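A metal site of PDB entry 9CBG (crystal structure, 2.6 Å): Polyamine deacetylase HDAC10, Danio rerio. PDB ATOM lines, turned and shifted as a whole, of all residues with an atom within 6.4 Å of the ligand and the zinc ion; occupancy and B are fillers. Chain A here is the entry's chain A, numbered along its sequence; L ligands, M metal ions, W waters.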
ATOM      1  N   PRO A  23      19.825  20.904  -3.747  1.00  0.00           N
ATOM      2  CA  PRO A  23      18.566  21.263  -3.067  1.00  0.00           C
ATOM      3  C   PRO A  23      18.775  21.878  -1.692  1.00  0.00           C
ATOM      4  O   PRO A  23      17.846  22.505  -1.167  1.00  0.00           O
ATOM      5  CB  PRO A  23      17.818  19.932  -2.978  1.00  0.00           C
ATOM      6  CG  PRO A  23      18.432  19.075  -4.051  1.00  0.00           C
ATOM      7  CD  PRO A  23      19.878  19.472  -4.080  1.00  0.00           C
ATOM      8  N   GLU A  24      19.966  21.740  -1.111  1.00  0.00           N
ATOM      9  CA  GLU A  24      20.223  22.324   0.199  1.00  0.00           C
ATOM     10  C   GLU A  24      20.450  23.830   0.111  1.00  0.00           C
ATOM     11  O   GLU A  24      20.048  24.569   1.025  1.00  0.00           O
ATOM     12  CB  GLU A  24      21.423  21.649   0.841  1.00  0.00           C
ATOM     13  CG  GLU A  24      21.603  21.957   2.311  1.00  0.00           C
ATOM     14  CD  GLU A  24      22.735  21.160   2.906  1.00  0.00           C
ATOM     15  OE1 GLU A  24      23.705  20.884   2.165  1.00  0.00           O
ATOM     16  OE2 GLU A  24      22.665  20.798   4.095  1.00  0.00           O
ATOM     17  N   CYS A  25      21.089  24.304  -0.954  1.00  0.00           N
ATOM     18  CA  CYS A  25      21.427  25.714  -1.123  1.00  0.00           C
ATOM     19  C   CYS A  25      20.511  26.440  -2.101  1.00  0.00           C
ATOM     20  O   CYS A  25      20.739  27.628  -2.378  1.00  0.00           O
ATOM     21  CB  CYS A  25      22.882  25.858  -1.570  1.00  0.00           C
ATOM     22  SG  CYS A  25      24.143  25.328  -0.386  1.00  0.00           S
ATOM     23  N   ILE A  27      17.723  27.768  -1.840  1.00  0.00           N
ATOM     24  CA  ILE A  27      16.916  28.869  -1.332  1.00  0.00           C
ATOM     25  C   ILE A  27      17.698  30.184  -1.325  1.00  0.00           C
ATOM     26  O   ILE A  27      17.091  31.257  -1.391  1.00  0.00           O
ATOM     27  CB  ILE A  27      16.396  28.541   0.081  1.00  0.00           C
ATOM     28  CG1 ILE A  27      17.562  28.190   1.012  1.00  0.00           C
ATOM     29  CG2 ILE A  27      15.353  27.433   0.028  1.00  0.00           C
ATOM     30  CD1 ILE A  27      17.190  28.119   2.475  1.00  0.00           C
ATOM     31  N   ASN A  93      30.222  22.422   4.586  1.00  0.00           N
ATOM     32  CA  ASN A  93      28.850  21.949   4.755  1.00  0.00           C
ATOM     33  C   ASN A  93      27.877  23.082   4.448  1.00  0.00           C
ATOM     34  O   ASN A  93      27.927  24.137   5.086  1.00  0.00           O
ATOM     35  CB  ASN A  93      28.621  21.400   6.165  1.00  0.00           C
ATOM     36  CG  ASN A  93      27.161  21.110   6.449  1.00  0.00           C
ATOM     37  OD1 ASN A  93      26.550  21.727   7.316  1.00  0.00           O
ATOM     38  ND2 ASN A  93      26.588  20.183   5.688  1.00  0.00           N
ATOM     39  N   ALA A  94      27.024  22.862   3.445  1.00  0.00           N
ATOM     40  CA  ALA A  94      25.905  23.755   3.116  1.00  0.00           C
ATOM     41  C   ALA A  94      26.371  25.130   2.627  1.00  0.00           C
ATOM     42  O   ALA A  94      25.920  26.169   3.111  1.00  0.00           O
ATOM     43  CB  ALA A  94      24.946  23.882   4.297  1.00  0.00           C
ATOM     44  N   PRO A 134      25.519  36.033   3.730  1.00  0.00           N
ATOM     45  CA  PRO A 134      25.388  36.150   5.186  1.00  0.00           C
ATOM     46  C   PRO A 134      26.683  35.797   5.904  1.00  0.00           C
ATOM     47  O   PRO A 134      27.689  35.455   5.269  1.00  0.00           O
ATOM     48  CB  PRO A 134      24.276  35.155   5.527  1.00  0.00           C
ATOM     49  CG  PRO A 134      23.650  34.757   4.236  1.00  0.00           C
ATOM     50  CD  PRO A 134      24.709  34.931   3.187  1.00  0.00           C
ATOM     51  N   HIS A 136      26.694  34.754   9.893  1.00  0.00           N
ATOM     52  CA  HIS A 136      26.711  34.287  11.288  1.00  0.00           C
ATOM     53  C   HIS A 136      27.115  32.828  11.433  1.00  0.00           C
ATOM     54  O   HIS A 136      27.370  32.394  12.569  1.00  0.00           O
ATOM     55  CB  HIS A 136      25.355  34.538  11.970  1.00  0.00           C
ATOM     56  CG  HIS A 136      24.224  33.722  11.416  1.00  0.00           C
ATOM     57  ND1 HIS A 136      23.161  33.315  12.187  1.00  0.00           N
ATOM     58  CD2 HIS A 136      23.966  33.284  10.157  1.00  0.00           C
ATOM     59  CE1 HIS A 136      22.302  32.644  11.441  1.00  0.00           C
ATOM     60  NE2 HIS A 136      22.771  32.613  10.205  1.00  0.00           N
ATOM     61  N   HIS A 137      27.196  32.062  10.348  1.00  0.00           N
ATOM     62  CA  HIS A 137      27.614  30.668  10.419  1.00  0.00           C
ATOM     63  C   HIS A 137      29.103  30.471  10.146  1.00  0.00           C
ATOM     64  O   HIS A 137      29.675  29.479  10.624  1.00  0.00           O
ATOM     65  CB  HIS A 137      26.818  29.812   9.426  1.00  0.00           C
ATOM     66  CG  HIS A 137      25.376  29.669   9.791  1.00  0.00           C
ATOM     67  ND1 HIS A 137      24.965  29.059  10.968  1.00  0.00           N
ATOM     68  CD2 HIS A 137      24.243  30.045   9.151  1.00  0.00           C
ATOM     69  CE1 HIS A 137      23.651  29.082  11.033  1.00  0.00           C
ATOM     70  NE2 HIS A 137      23.185  29.673   9.945  1.00  0.00           N
ATOM     71  N   ASN A 144      30.486  28.213   6.094  1.00  0.00           N
ATOM     72  CA  ASN A 144      29.394  27.325   6.567  1.00  0.00           C
ATOM     73  C   ASN A 144      28.057  28.025   6.439  1.00  0.00           C
ATOM     74  O   ASN A 144      28.015  29.236   6.666  1.00  0.00           O
ATOM     75  CB  ASN A 144      29.640  26.918   8.023  1.00  0.00           C
ATOM     76  CG  ASN A 144      28.686  25.869   8.521  1.00  0.00           C
ATOM     77  OD1 ASN A 144      27.919  26.131   9.450  1.00  0.00           O
ATOM     78  ND2 ASN A 144      28.716  24.685   7.921  1.00  0.00           N
ATOM     79  N   GLY A 145      27.014  27.302   6.050  1.00  0.00           N
ATOM     80  CA  GLY A 145      25.654  27.884   6.039  1.00  0.00           C
ATOM     81  C   GLY A 145      25.546  29.107   5.180  1.00  0.00           C
ATOM     82  O   GLY A 145      25.186  30.165   5.722  1.00  0.00           O
ATOM     83  N   PHE A 146      25.849  28.968   3.894  1.00  0.00           N
ATOM     84  CA  PHE A 146      25.701  30.093   2.931  1.00  0.00           C
ATOM     85  C   PHE A 146      26.576  31.264   3.358  1.00  0.00           C
ATOM     86  O   PHE A 146      26.426  32.346   2.783  1.00  0.00           O
ATOM     87  CB  PHE A 146      24.240  30.516   2.820  1.00  0.00           C
ATOM     88  CG  PHE A 146      23.156  29.453   2.706  1.00  0.00           C
ATOM     89  CD1 PHE A 146      23.395  28.240   2.073  1.00  0.00           C
ATOM     90  CD2 PHE A 146      21.885  29.687   3.219  1.00  0.00           C
ATOM     91  CE1 PHE A 146      22.398  27.290   1.968  1.00  0.00           C
ATOM     92  CE2 PHE A 146      20.897  28.725   3.115  1.00  0.00           C
ATOM     93  CZ  PHE A 146      21.150  27.542   2.487  1.00  0.00           C
ATOM     94  N   CYS A 147      27.469  31.067   4.326  1.00  0.00           N
ATOM     95  CA  CYS A 147      28.281  32.168   4.818  1.00  0.00           C
ATOM     96  C   CYS A 147      29.744  31.974   4.442  1.00  0.00           C
ATOM     97  O   CYS A 147      30.273  30.851   4.508  1.00  0.00           O
ATOM     98  CB  CYS A 147      28.162  32.319   6.348  1.00  0.00           C
ATOM     99  SG  CYS A 147      26.504  32.696   6.960  1.00  0.00           S
ATOM    100  N   ASP A 174      17.770  35.114  13.787  1.00  0.00           N
ATOM    101  CA  ASP A 174      17.661  34.097  12.742  1.00  0.00           C
ATOM    102  C   ASP A 174      17.313  32.742  13.370  1.00  0.00           C
ATOM    103  O   ASP A 174      17.742  32.455  14.497  1.00  0.00           O
ATOM    104  CB  ASP A 174      18.993  34.012  11.995  1.00  0.00           C
ATOM    105  CG  ASP A 174      18.908  33.228  10.697  1.00  0.00           C
ATOM    106  OD1 ASP A 174      18.606  32.022  10.732  1.00  0.00           O
ATOM    107  OD2 ASP A 174      19.150  33.829   9.644  1.00  0.00           O
ATOM    108  N   VAL A 175      16.530  31.911  12.659  1.00  0.00           N
ATOM    109  CA  VAL A 175      16.152  30.610  13.224  1.00  0.00           C
ATOM    110  C   VAL A 175      17.334  29.676  13.348  1.00  0.00           C
ATOM    111  O   VAL A 175      17.224  28.629  13.995  1.00  0.00           O
ATOM    112  CB  VAL A 175      15.079  29.848  12.424  1.00  0.00           C
ATOM    113  CG1 VAL A 175      13.678  30.361  12.693  1.00  0.00           C
ATOM    114  CG2 VAL A 175      15.428  29.827  10.950  1.00  0.00           C
ATOM    115  N   HIS A 176      18.449  30.080  12.752  1.00  0.00           N
ATOM    116  CA  HIS A 176      19.669  29.250  12.814  1.00  0.00           C
ATOM    117  C   HIS A 176      20.592  29.825  13.886  1.00  0.00           C
ATOM    118  O   HIS A 176      20.429  31.003  14.262  1.00  0.00           O
ATOM    119  CB  HIS A 176      20.284  29.131  11.413  1.00  0.00           C
ATOM    120  CG  HIS A 176      19.362  28.579  10.397  1.00  0.00           C
ATOM    121  ND1 HIS A 176      18.577  29.329   9.539  1.00  0.00           N
ATOM    122  CD2 HIS A 176      19.114  27.305  10.100  1.00  0.00           C
ATOM    123  CE1 HIS A 176      17.866  28.499   8.787  1.00  0.00           C
ATOM    124  NE2 HIS A 176      18.197  27.272   9.098  1.00  0.00           N
ATOM    125  N   PHE A 204      18.000  19.441  14.076  1.00  0.00           N
ATOM    126  CA  PHE A 204      17.931  20.467  13.043  1.00  0.00           C
ATOM    127  C   PHE A 204      19.290  21.116  12.817  1.00  0.00           C
ATOM    128  O   PHE A 204      20.105  21.263  13.743  1.00  0.00           O
ATOM    129  CB  PHE A 204      16.902  21.542  13.412  1.00  0.00           C
ATOM    130  CG  PHE A 204      16.615  22.512  12.297  1.00  0.00           C
ATOM    131  CD1 PHE A 204      15.772  22.150  11.263  1.00  0.00           C
ATOM    132  CD2 PHE A 204      17.187  23.773  12.284  1.00  0.00           C
ATOM    133  CE1 PHE A 204      15.499  23.032  10.228  1.00  0.00           C
ATOM    134  CE2 PHE A 204      16.925  24.665  11.257  1.00  0.00           C
ATOM    135  CZ  PHE A 204      16.070  24.285  10.226  1.00  0.00           C
ATOM    136  N   TRP A 205      19.523  21.532  11.567  1.00  0.00           N
ATOM    137  CA  TRP A 205      20.820  22.051  11.163  1.00  0.00           C
ATOM    138  C   TRP A 205      21.181  23.275  12.003  1.00  0.00           C
ATOM    139  O   TRP A 205      20.328  24.133  12.256  1.00  0.00           O
ATOM    140  CB  TRP A 205      20.810  22.405   9.679  1.00  0.00           C
ATOM    141  CG  TRP A 205      22.183  22.648   9.149  1.00  0.00           C
ATOM    142  CD1 TRP A 205      23.002  21.734   8.551  1.00  0.00           C
ATOM    143  CD2 TRP A 205      22.910  23.877   9.195  1.00  0.00           C
ATOM    144  NE1 TRP A 205      24.194  22.316   8.225  1.00  0.00           N
ATOM    145  CE2 TRP A 205      24.171  23.630   8.613  1.00  0.00           C
ATOM    146  CE3 TRP A 205      22.624  25.149   9.682  1.00  0.00           C
ATOM    147  CZ2 TRP A 205      25.142  24.621   8.496  1.00  0.00           C
ATOM    148  CZ3 TRP A 205      23.584  26.132   9.566  1.00  0.00           C
ATOM    149  CH2 TRP A 205      24.833  25.865   8.979  1.00  0.00           C
ATOM    150  N   GLY A 265      18.137  37.834  10.646  1.00  0.00           N
ATOM    151  CA  GLY A 265      17.654  36.747   9.827  1.00  0.00           C
ATOM    152  C   GLY A 265      16.157  36.643   9.938  1.00  0.00           C
ATOM    153  O   GLY A 265      15.629  36.373  11.022  1.00  0.00           O
ATOM    154  N   ASP A 267      14.192  34.459   8.438  1.00  0.00           N
ATOM    155  CA  ASP A 267      13.623  33.113   8.296  1.00  0.00           C
ATOM    156  C   ASP A 267      12.890  32.662   9.548  1.00  0.00           C
ATOM    157  O   ASP A 267      12.321  31.565   9.559  1.00  0.00           O
ATOM    158  CB  ASP A 267      14.712  32.100   7.924  1.00  0.00           C
ATOM    159  CG  ASP A 267      15.960  32.217   8.779  1.00  0.00           C
ATOM    160  OD1 ASP A 267      15.941  32.965   9.777  1.00  0.00           O
ATOM    161  OD2 ASP A 267      16.966  31.546   8.448  1.00  0.00           O
ATOM    162  N   GLU A 274      12.216  27.478   5.581  1.00  0.00           N
ATOM    163  CA  GLU A 274      13.291  26.882   6.358  1.00  0.00           C
ATOM    164  C   GLU A 274      12.970  26.893   7.855  1.00  0.00           C
ATOM    165  O   GLU A 274      13.125  25.872   8.530  1.00  0.00           O
ATOM    166  CB  GLU A 274      14.595  27.621   6.072  1.00  0.00           C
ATOM    167  CG  GLU A 274      15.830  26.960   6.660  1.00  0.00           C
ATOM    168  CD  GLU A 274      16.145  25.637   6.000  1.00  0.00           C
ATOM    169  OE1 GLU A 274      15.897  25.485   4.783  1.00  0.00           O
ATOM    170  OE2 GLU A 274      16.640  24.736   6.713  1.00  0.00           O
ATOM    171  N   GLU A 304      20.861  38.601   7.597  1.00  0.00           N
ATOM    172  CA  GLU A 304      21.436  37.239   7.642  1.00  0.00           C
ATOM    173  C   GLU A 304      20.546  36.332   6.782  1.00  0.00           C
ATOM    174  O   GLU A 304      20.836  36.193   5.587  1.00  0.00           O
ATOM    175  CB  GLU A 304      21.548  36.744   9.074  1.00  0.00           C
ATOM    176  CG  GLU A 304      22.588  37.496   9.897  1.00  0.00           C
ATOM    177  CD  GLU A 304      24.017  37.045   9.697  1.00  0.00           C
ATOM    178  OE1 GLU A 304      24.259  36.144   8.876  1.00  0.00           O
ATOM    179  OE2 GLU A 304      24.901  37.595  10.376  1.00  0.00           O
ATOM    180  N   GLY A 305      19.479  35.772   7.360  1.00  0.00           N
ATOM    181  CA  GLY A 305      18.638  34.820   6.622  1.00  0.00           C
ATOM    182  C   GLY A 305      17.287  35.364   6.231  1.00  0.00           C
ATOM    183  O   GLY A 305      17.052  36.560   6.439  1.00  0.00           O
ATOM    184  N   GLY A 306      16.423  34.510   5.697  1.00  0.00           N
ATOM    185  CA  GLY A 306      15.129  34.926   5.181  1.00  0.00           C
ATOM    186  C   GLY A 306      14.924  34.582   3.718  1.00  0.00           C
ATOM    187  O   GLY A 306      15.519  35.224   2.833  1.00  0.00           O
ATOM    188  N   TYR A 307      14.060  33.594   3.437  1.00  0.00           N
ATOM    189  CA  TYR A 307      13.995  33.006   2.099  1.00  0.00           C
ATOM    190  C   TYR A 307      12.602  32.934   1.499  1.00  0.00           C
ATOM    191  O   TYR A 307      12.446  32.408   0.392  1.00  0.00           O
ATOM    192  CB  TYR A 307      14.626  31.609   2.121  1.00  0.00           C
ATOM    193  CG  TYR A 307      15.979  31.630   2.792  1.00  0.00           C
ATOM    194  CD1 TYR A 307      17.126  31.941   2.073  1.00  0.00           C
ATOM    195  CD2 TYR A 307      16.116  31.353   4.149  1.00  0.00           C
ATOM    196  CE1 TYR A 307      18.370  31.966   2.681  1.00  0.00           C
ATOM    197  CE2 TYR A 307      17.349  31.371   4.769  1.00  0.00           C
ATOM    198  CZ  TYR A 307      18.467  31.683   4.028  1.00  0.00           C
ATOM    199  OH  TYR A 307      19.698  31.694   4.660  1.00  0.00           O
HETATM  200  C1  LIG L   1      20.527  29.114   6.494  1.00  0.00           C
HETATM  201  C2  LIG L   1      21.577  30.194   6.768  1.00  0.00           C
HETATM  202  C3  LIG L   1      20.988  27.666   6.291  1.00  0.00           C
HETATM  203  C4  LIG L   1      20.076  26.646   6.067  1.00  0.00           C
HETATM  204  C5  LIG L   1      20.527  25.341   5.895  1.00  0.00           C
HETATM  205  C6  LIG L   1      19.538  24.206   5.654  1.00  0.00           C
HETATM  206  C7  LIG L   1      19.126  24.039   4.193  1.00  0.00           C
HETATM  207  C8  LIG L   1      21.888  25.056   5.946  1.00  0.00           C
HETATM  208  C9  LIG L   1      22.790  26.077   6.169  1.00  0.00           C
HETATM  209  C10 LIG L   1      22.350  27.380   6.341  1.00  0.00           C
HETATM  210  N1  LIG L   1      17.869  23.324   4.128  1.00  0.00           N
HETATM  211  O1  LIG L   1      19.377  29.398   6.446  1.00  0.00           O
HETATM  212  S1  LIG L   1      21.004  31.371   8.018  1.00  0.00           S
HETATM  213 ZN    ZN M   1      18.941  31.336   8.877  1.00  0.00          ZN
HETATM  214  O   HOH W   1      16.947  24.219   1.624  1.00  0.00           O
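The zinc ion is bound by the side-chain carboxylate (OD1) of Asp 174, the side-chain carboxylate (OD2) of Asp 267, a ring nitrogen (ND1) of His 176 and a sulfur (S1) of the ligand. Slightly farther from the zinc ion lies the side-chain carboxylate (OD2) of Asp 174 (2.6 Å).
Water W1 lies within hydrogen-bond range of N1 of the ligand (2.8 Å), O of Glu 24 (3.2 Å) and O of Pro 23 (3.4 Å).
OE1 of Glu 274 lies within salt-bridge range of N1 of the ligand, 3.0 Å away. The side-chain hydroxyl (OH) of Tyr 307 sits at hydrogen-bond distance from an oxygen (O1) of the ligand. A ring nitrogen (NE2) of His 137 lies close to a sulfur (S1) of the ligand (3.4 Å). NE2 of His 136 sits close to S1 of the ligand, 3.1 Å away.
Residues that only touch the ligand: Glu 24, Ala 94, Gly 145, Phe 146 and Trp 205. Hydrophobic or aromatic side chains that line the ligand: Ala 94, His 136, His 137, Phe 146, His 176, Trp 205 and Tyr 307. Of the 25 residues printed, 12 come within 4 Å of the ligand.
O of Gly 145 lies within hydrogen-bond range of SG of Cys 147. OD1 of Asp 267 is in hydrogen-bond range of N of Val 175, at 3.1 Å. The side-chain carboxylate (OD2) of Asp 174 is in hydrogen-bond range of the backbone NH (N) of Gly 305, at 3.0 Å. The backbone carbonyl oxygen (O) of Asn 93 sits at hydrogen-bond distance from the backbone NH (N) of Gly 145 (3.4 Å). The backbone NH (N) of Gly 145 lies within hydrogen-bond range of the backbone carbonyl oxygen (O) of Ala 94 (3.3 Å). N of His 136 sits at hydrogen-bond distance from SG of Cys 147 (3.6 Å). A ring nitrogen (NE2) of His 137 sits at hydrogen-bond distance from a ring nitrogen (NE2) of His 136, at 3.0 Å. The backbone carbonyl oxygen (O) of Ala 94 is in hydrogen-bond range of the backbone NH (N) of Phe 146 (2.9 Å).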
